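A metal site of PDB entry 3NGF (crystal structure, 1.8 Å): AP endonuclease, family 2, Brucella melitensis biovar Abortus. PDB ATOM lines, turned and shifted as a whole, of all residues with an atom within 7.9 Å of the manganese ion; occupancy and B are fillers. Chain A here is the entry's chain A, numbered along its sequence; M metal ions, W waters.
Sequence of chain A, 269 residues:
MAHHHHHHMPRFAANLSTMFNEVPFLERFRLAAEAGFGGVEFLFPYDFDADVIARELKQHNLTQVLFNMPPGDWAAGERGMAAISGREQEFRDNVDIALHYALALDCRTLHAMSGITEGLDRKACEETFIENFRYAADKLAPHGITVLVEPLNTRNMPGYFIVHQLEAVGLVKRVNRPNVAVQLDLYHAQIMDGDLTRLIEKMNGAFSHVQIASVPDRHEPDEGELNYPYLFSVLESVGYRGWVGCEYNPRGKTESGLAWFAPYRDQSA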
ATOM      1  N   ASN A  15      24.188  11.406   8.439  1.00  0.00           N
ATOM      2  CA  ASN A  15      22.820  10.905   8.535  1.00  0.00           C
ATOM      3  C   ASN A  15      22.619   9.695   7.611  1.00  0.00           C
ATOM      4  O   ASN A  15      22.608   9.819   6.379  1.00  0.00           O
ATOM      5  CB  ASN A  15      21.786  12.015   8.262  1.00  0.00           C
ATOM      6  CG  ASN A  15      20.374  11.574   8.548  1.00  0.00           C
ATOM      7  OD1 ASN A  15      19.914  10.610   7.952  1.00  0.00           O
ATOM      8  ND2 ASN A  15      19.690  12.269   9.475  1.00  0.00           N
ATOM      9  N   GLU A  41      23.746   9.592  12.727  1.00  0.00           N
ATOM     10  CA  GLU A  41      22.351   9.773  13.130  1.00  0.00           C
ATOM     11  C   GLU A  41      21.485   9.101  12.086  1.00  0.00           C
ATOM     12  O   GLU A  41      21.945   8.842  10.965  1.00  0.00           O
ATOM     13  CB  GLU A  41      21.993  11.248  13.257  1.00  0.00           C
ATOM     14  CG  GLU A  41      22.070  12.055  11.951  1.00  0.00           C
ATOM     15  CD  GLU A  41      21.701  13.511  12.131  1.00  0.00           C
ATOM     16  OE1 GLU A  41      21.911  14.060  13.240  1.00  0.00           O
ATOM     17  OE2 GLU A  41      21.194  14.109  11.143  1.00  0.00           O
ATOM     18  N   LEU A  43      16.791   8.418  11.285  1.00  0.00           N
ATOM     19  CA  LEU A  43      15.458   8.676  11.840  1.00  0.00           C
ATOM     20  C   LEU A  43      14.992   7.561  12.759  1.00  0.00           C
ATOM     21  O   LEU A  43      14.815   7.775  13.970  1.00  0.00           O
ATOM     22  CB  LEU A  43      14.458   8.939  10.706  1.00  0.00           C
ATOM     23  CG  LEU A  43      14.588  10.355  10.165  1.00  0.00           C
ATOM     24  CD1 LEU A  43      15.797  10.494   9.321  1.00  0.00           C
ATOM     25  CD2 LEU A  43      13.316  10.802   9.418  1.00  0.00           C
ATOM     26  N   LEU A  66      21.992  10.772  17.531  1.00  0.00           N
ATOM     27  CA  LEU A  66      20.569  11.155  17.515  1.00  0.00           C
ATOM     28  C   LEU A  66      19.750  10.089  16.809  1.00  0.00           C
ATOM     29  O   LEU A  66      20.230   9.480  15.846  1.00  0.00           O
ATOM     30  CB  LEU A  66      20.376  12.505  16.793  1.00  0.00           C
ATOM     31  CG  LEU A  66      18.909  12.981  16.615  1.00  0.00           C
ATOM     32  CD1 LEU A  66      18.464  13.617  17.879  1.00  0.00           C
ATOM     33  CD2 LEU A  66      18.765  13.935  15.418  1.00  0.00           C
ATOM     34  N   ASN A  68      15.060   9.349  16.250  1.00  0.00           N
ATOM     35  CA  ASN A  68      13.702   9.794  16.608  1.00  0.00           C
ATOM     36  C   ASN A  68      12.957   8.726  17.373  1.00  0.00           C
ATOM     37  O   ASN A  68      13.140   7.525  17.145  1.00  0.00           O
ATOM     38  CB  ASN A  68      12.886  10.113  15.368  1.00  0.00           C
ATOM     39  CG  ASN A  68      13.444  11.225  14.541  1.00  0.00           C
ATOM     40  OD1 ASN A  68      14.481  11.800  14.862  1.00  0.00           O
ATOM     41  ND2 ASN A  68      12.752  11.551  13.433  1.00  0.00           N
ATOM     42  N   HIS A 111      14.866  12.778  19.399  1.00  0.00           N
ATOM     43  CA  HIS A 111      13.890  13.714  18.854  1.00  0.00           C
ATOM     44  C   HIS A 111      12.470  13.120  18.979  1.00  0.00           C
ATOM     45  O   HIS A 111      12.189  12.043  18.418  1.00  0.00           O
ATOM     46  CB  HIS A 111      14.257  14.045  17.406  1.00  0.00           C
ATOM     47  CG  HIS A 111      13.212  14.795  16.637  1.00  0.00           C
ATOM     48  ND1 HIS A 111      13.129  14.732  15.260  1.00  0.00           N
ATOM     49  CD2 HIS A 111      12.217  15.620  17.040  1.00  0.00           C
ATOM     50  CE1 HIS A 111      12.145  15.505  14.847  1.00  0.00           C
ATOM     51  NE2 HIS A 111      11.573  16.054  15.903  1.00  0.00           N
ATOM     52  N   GLU A 150      11.998  19.561  17.169  1.00  0.00           N
ATOM     53  CA  GLU A 150      12.607  20.074  15.925  1.00  0.00           C
ATOM     54  C   GLU A 150      11.612  20.842  15.079  1.00  0.00           C
ATOM     55  O   GLU A 150      10.735  20.235  14.457  1.00  0.00           O
ATOM     56  CB  GLU A 150      13.149  18.965  15.053  1.00  0.00           C
ATOM     57  CG  GLU A 150      14.010  19.492  13.902  1.00  0.00           C
ATOM     58  CD  GLU A 150      14.362  18.471  12.822  1.00  0.00           C
ATOM     59  OE1 GLU A 150      13.928  17.308  12.831  1.00  0.00           O
ATOM     60  OE2 GLU A 150      15.117  18.878  11.927  1.00  0.00           O
ATOM     61  N   PRO A 151      11.745  22.174  15.033  1.00  0.00           N
ATOM     62  CA  PRO A 151      10.944  22.923  14.045  1.00  0.00           C
ATOM     63  C   PRO A 151      11.267  22.473  12.620  1.00  0.00           C
ATOM     64  O   PRO A 151      12.437  22.317  12.267  1.00  0.00           O
ATOM     65  CB  PRO A 151      11.376  24.383  14.275  1.00  0.00           C
ATOM     66  CG  PRO A 151      11.890  24.396  15.675  1.00  0.00           C
ATOM     67  CD  PRO A 151      12.531  23.059  15.889  1.00  0.00           C
ATOM     68  N   LEU A 152      10.223  22.280  11.824  1.00  0.00           N
ATOM     69  CA  LEU A 152      10.373  21.892  10.427  1.00  0.00           C
ATOM     70  C   LEU A 152      10.055  23.116   9.543  1.00  0.00           C
ATOM     71  O   LEU A 152      10.270  24.261   9.967  1.00  0.00           O
ATOM     72  CB  LEU A 152       9.559  20.642  10.147  1.00  0.00           C
ATOM     73  CG  LEU A 152       9.905  19.440  11.055  1.00  0.00           C
ATOM     74  CD1 LEU A 152       9.076  18.213  10.666  1.00  0.00           C
ATOM     75  CD2 LEU A 152      11.429  19.102  11.029  1.00  0.00           C
ATOM     76  N   GLN A 183      16.130  21.110  18.599  1.00  0.00           N
ATOM     77  CA  GLN A 183      16.973  20.585  17.534  1.00  0.00           C
ATOM     78  C   GLN A 183      16.951  21.628  16.403  1.00  0.00           C
ATOM     79  O   GLN A 183      15.919  21.836  15.770  1.00  0.00           O
ATOM     80  CB  GLN A 183      16.422  19.246  17.064  1.00  0.00           C
ATOM     81  CG  GLN A 183      17.198  18.558  15.936  1.00  0.00           C
ATOM     82  CD  GLN A 183      16.725  17.148  15.703  1.00  0.00           C
ATOM     83  OE1 GLN A 183      16.344  16.455  16.628  1.00  0.00           O
ATOM     84  NE2 GLN A 183      16.778  16.703  14.456  1.00  0.00           N
ATOM     85  N   LEU A 184      18.073  22.302  16.208  1.00  0.00           N
ATOM     86  CA  LEU A 184      18.196  23.425  15.250  1.00  0.00           C
ATOM     87  C   LEU A 184      18.732  22.916  13.907  1.00  0.00           C
ATOM     88  O   LEU A 184      19.953  22.750  13.730  1.00  0.00           O
ATOM     89  CB  LEU A 184      19.142  24.471  15.856  1.00  0.00           C
ATOM     90  CG  LEU A 184      19.515  25.700  15.038  1.00  0.00           C
ATOM     91  CD1 LEU A 184      18.267  26.412  14.524  1.00  0.00           C
ATOM     92  CD2 LEU A 184      20.444  26.658  15.826  1.00  0.00           C
ATOM     93  N   ASP A 185      17.817  22.629  12.990  1.00  0.00           N
ATOM     94  CA  ASP A 185      18.153  22.243  11.614  1.00  0.00           C
ATOM     95  C   ASP A 185      18.173  23.554  10.794  1.00  0.00           C
ATOM     96  O   ASP A 185      17.136  24.254  10.636  1.00  0.00           O
ATOM     97  CB  ASP A 185      17.133  21.214  11.119  1.00  0.00           C
ATOM     98  CG  ASP A 185      17.383  20.721   9.705  1.00  0.00           C
ATOM     99  OD1 ASP A 185      17.883  21.491   8.891  1.00  0.00           O
ATOM    100  OD2 ASP A 185      17.025  19.570   9.364  1.00  0.00           O
ATOM    101  N   LEU A 186      19.377  23.925  10.346  1.00  0.00           N
ATOM    102  CA  LEU A 186      19.558  25.268   9.774  1.00  0.00           C
ATOM    103  C   LEU A 186      18.894  25.374   8.417  1.00  0.00           C
ATOM    104  O   LEU A 186      18.575  26.482   7.923  1.00  0.00           O
ATOM    105  CB  LEU A 186      21.052  25.616   9.720  1.00  0.00           C
ATOM    106  CG  LEU A 186      21.694  25.846  11.079  1.00  0.00           C
ATOM    107  CD1 LEU A 186      23.204  25.959  10.949  1.00  0.00           C
ATOM    108  CD2 LEU A 186      21.095  27.109  11.775  1.00  0.00           C
ATOM    109  N   TYR A 187      18.690  24.226   7.778  1.00  0.00           N
ATOM    110  CA  TYR A 187      17.911  24.182   6.539  1.00  0.00           C
ATOM    111  C   TYR A 187      16.464  24.690   6.826  1.00  0.00           C
ATOM    112  O   TYR A 187      15.940  25.587   6.135  1.00  0.00           O
ATOM    113  CB  TYR A 187      17.933  22.746   5.978  1.00  0.00           C
ATOM    114  CG  TYR A 187      16.965  22.466   4.857  1.00  0.00           C
ATOM    115  CD1 TYR A 187      17.267  22.781   3.544  1.00  0.00           C
ATOM    116  CD2 TYR A 187      15.730  21.884   5.115  1.00  0.00           C
ATOM    117  CE1 TYR A 187      16.359  22.549   2.498  1.00  0.00           C
ATOM    118  CE2 TYR A 187      14.831  21.620   4.094  1.00  0.00           C
ATOM    119  CZ  TYR A 187      15.128  21.972   2.799  1.00  0.00           C
ATOM    120  OH  TYR A 187      14.211  21.707   1.808  1.00  0.00           O
ATOM    121  N   HIS A 188      15.842  24.133   7.854  1.00  0.00           N
ATOM    122  CA  HIS A 188      14.490  24.550   8.215  1.00  0.00           C
ATOM    123  C   HIS A 188      14.471  26.006   8.738  1.00  0.00           C
ATOM    124  O   HIS A 188      13.556  26.746   8.437  1.00  0.00           O
ATOM    125  CB  HIS A 188      13.902  23.604   9.261  1.00  0.00           C
ATOM    126  CG  HIS A 188      13.689  22.200   8.772  1.00  0.00           C
ATOM    127  ND1 HIS A 188      13.047  21.900   7.592  1.00  0.00           N
ATOM    128  CD2 HIS A 188      13.963  21.006   9.364  1.00  0.00           C
ATOM    129  CE1 HIS A 188      12.956  20.582   7.469  1.00  0.00           C
ATOM    130  NE2 HIS A 188      13.524  20.017   8.520  1.00  0.00           N
ATOM    131  N   HIS A 209      21.333  20.037  19.441  1.00  0.00           N
ATOM    132  CA  HIS A 209      21.733  19.389  18.217  1.00  0.00           C
ATOM    133  C   HIS A 209      21.486  20.387  17.095  1.00  0.00           C
ATOM    134  O   HIS A 209      20.590  21.224  17.182  1.00  0.00           O
ATOM    135  CB  HIS A 209      20.955  18.085  17.990  1.00  0.00           C
ATOM    136  CG  HIS A 209      21.530  17.230  16.895  1.00  0.00           C
ATOM    137  ND1 HIS A 209      22.831  16.786  16.905  1.00  0.00           N
ATOM    138  CD2 HIS A 209      20.982  16.770  15.746  1.00  0.00           C
ATOM    139  CE1 HIS A 209      23.069  16.087  15.799  1.00  0.00           C
ATOM    140  NE2 HIS A 209      21.959  16.069  15.082  1.00  0.00           N
ATOM    141  N   VAL A 210      22.306  20.274  16.066  1.00  0.00           N
ATOM    142  CA  VAL A 210      22.268  21.106  14.888  1.00  0.00           C
ATOM    143  C   VAL A 210      22.300  20.149  13.690  1.00  0.00           C
ATOM    144  O   VAL A 210      22.940  19.107  13.737  1.00  0.00           O
ATOM    145  CB  VAL A 210      23.446  22.102  14.846  1.00  0.00           C
ATOM    146  CG1 VAL A 210      23.470  22.894  13.489  1.00  0.00           C
ATOM    147  CG2 VAL A 210      23.405  23.051  16.038  1.00  0.00           C
ATOM    148  N   GLN A 211      21.570  20.495  12.647  1.00  0.00           N
ATOM    149  CA  GLN A 211      21.616  19.800  11.370  1.00  0.00           C
ATOM    150  C   GLN A 211      21.816  20.808  10.247  1.00  0.00           C
ATOM    151  O   GLN A 211      21.486  21.995  10.410  1.00  0.00           O
ATOM    152  CB  GLN A 211      20.343  18.999  11.135  1.00  0.00           C
ATOM    153  CG  GLN A 211      20.248  17.753  12.039  1.00  0.00           C
ATOM    154  CD  GLN A 211      18.896  17.106  11.922  1.00  0.00           C
ATOM    155  OE1 GLN A 211      17.886  17.788  11.899  1.00  0.00           O
ATOM    156  NE2 GLN A 211      18.881  15.785  11.829  1.00  0.00           N
ATOM    157  N   ILE A 212      22.402  20.323   9.148  1.00  0.00           N
ATOM    158  CA  ILE A 212      22.716  21.139   7.973  1.00  0.00           C
ATOM    159  C   ILE A 212      22.377  20.450   6.640  1.00  0.00           C
ATOM    160  O   ILE A 212      22.402  19.219   6.506  1.00  0.00           O
ATOM    161  CB  ILE A 212      24.213  21.592   7.950  1.00  0.00           C
ATOM    162  CG1 ILE A 212      25.166  20.394   7.754  1.00  0.00           C
ATOM    163  CG2 ILE A 212      24.554  22.398   9.221  1.00  0.00           C
ATOM    164  CD1 ILE A 212      26.654  20.800   7.552  1.00  0.00           C
ATOM    165  N   ARG A 218      18.671  21.144  -0.599  1.00  0.00           N
ATOM    166  CA  ARG A 218      18.864  20.129   0.458  1.00  0.00           C
ATOM    167  C   ARG A 218      19.931  19.104   0.085  1.00  0.00           C
ATOM    168  O   ARG A 218      19.779  17.915   0.317  1.00  0.00           O
ATOM    169  CB  ARG A 218      17.530  19.487   0.838  1.00  0.00           C
ATOM    170  CG  ARG A 218      17.466  19.015   2.292  1.00  0.00           C
ATOM    171  CD  ARG A 218      16.085  18.517   2.681  1.00  0.00           C
ATOM    172  NE  ARG A 218      16.029  18.263   4.125  1.00  0.00           N
ATOM    173  CZ  ARG A 218      14.919  17.946   4.803  1.00  0.00           C
ATOM    174  NH1 ARG A 218      13.767  17.762   4.171  1.00  0.00           N
ATOM    175  NH2 ARG A 218      14.989  17.761   6.101  1.00  0.00           N
ATOM    176  N   GLY A 245      24.608  17.319  12.508  1.00  0.00           N
ATOM    177  CA  GLY A 245      24.079  16.227  11.682  1.00  0.00           C
ATOM    178  C   GLY A 245      23.984  16.608  10.208  1.00  0.00           C
ATOM    179  O   GLY A 245      23.486  17.674   9.883  1.00  0.00           O
ATOM    180  N   GLU A 247      22.052  15.971   7.431  1.00  0.00           N
ATOM    181  CA  GLU A 247      20.785  15.503   6.953  1.00  0.00           C
ATOM    182  C   GLU A 247      20.515  16.172   5.597  1.00  0.00           C
ATOM    183  O   GLU A 247      19.657  17.085   5.487  1.00  0.00           O
ATOM    184  CB  GLU A 247      19.680  15.852   7.929  1.00  0.00           C
ATOM    185  CG  GLU A 247      18.399  15.148   7.591  1.00  0.00           C
ATOM    186  CD  GLU A 247      17.256  15.546   8.472  1.00  0.00           C
ATOM    187  OE1 GLU A 247      17.340  16.595   9.152  1.00  0.00           O
ATOM    188  OE2 GLU A 247      16.272  14.802   8.472  1.00  0.00           O
HETATM  189 MN    MN M   1      16.162  17.793  10.385  1.00  0.00          MN
HETATM  190  O   HOH W   1      15.346  15.784  11.549  1.00  0.00           O
HETATM  191  O   HOH W   2      14.367  17.444   9.037  1.00  0.00           O
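N of Glu 247 is in hydrogen-bond range of O of Ile 212 (3.4 Å). OE1 of Glu 150 is in hydrogen-bond range of NE2 of Gln 183, at 3.3 Å. N of His 188 is in hydrogen-bond range of OD1 of Asp 185 (3.5 Å). The backbone NH (N) of Tyr 187 sits at hydrogen-bond distance from the side-chain carboxylate (OD1) of Asp 185 (3.1 Å). NE2 of Gln 183 lies close to NE2 of Gln 211. NE2 of Gln 211 sits at hydrogen-bond distance from OE2 of Glu 41, 2.9 Å away. N of Gln 211 sits at hydrogen-bond distance from O of Leu 184 (3.0 Å). O of Gln 211 is in hydrogen-bond range of N of Leu 186 (2.9 Å).
Residues that only touch the manganese ion: His 188. Of the 22 residues printed, 5 come within 4 Å of the manganese ion.
The manganese ion is bound by OE1 of Glu 247 (2.1 Å), OE2 of Glu 150 (2.2 Å), OD2 of Asp 185 (2.2 Å), water W2 (2.3 Å), OE1 of Gln 211 (2.3 Å) and water W1 (2.5 Å). The manganese ion has six donor atoms within binding distance.
Water W2 lies within hydrogen-bond range of a ring nitrogen (NE2) of His 188 (2.8 Å), the guanidinium group of Arg 218 (3.0 Å) and the side-chain carboxylate of Glu 247 (3.3 Å). Water W1 lies within hydrogen-bond range of OE1 of Glu 150 (2.4 Å), OE2 of Glu 247 (3.4 Å) and NE2 of Gln 183 (3.4 Å).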
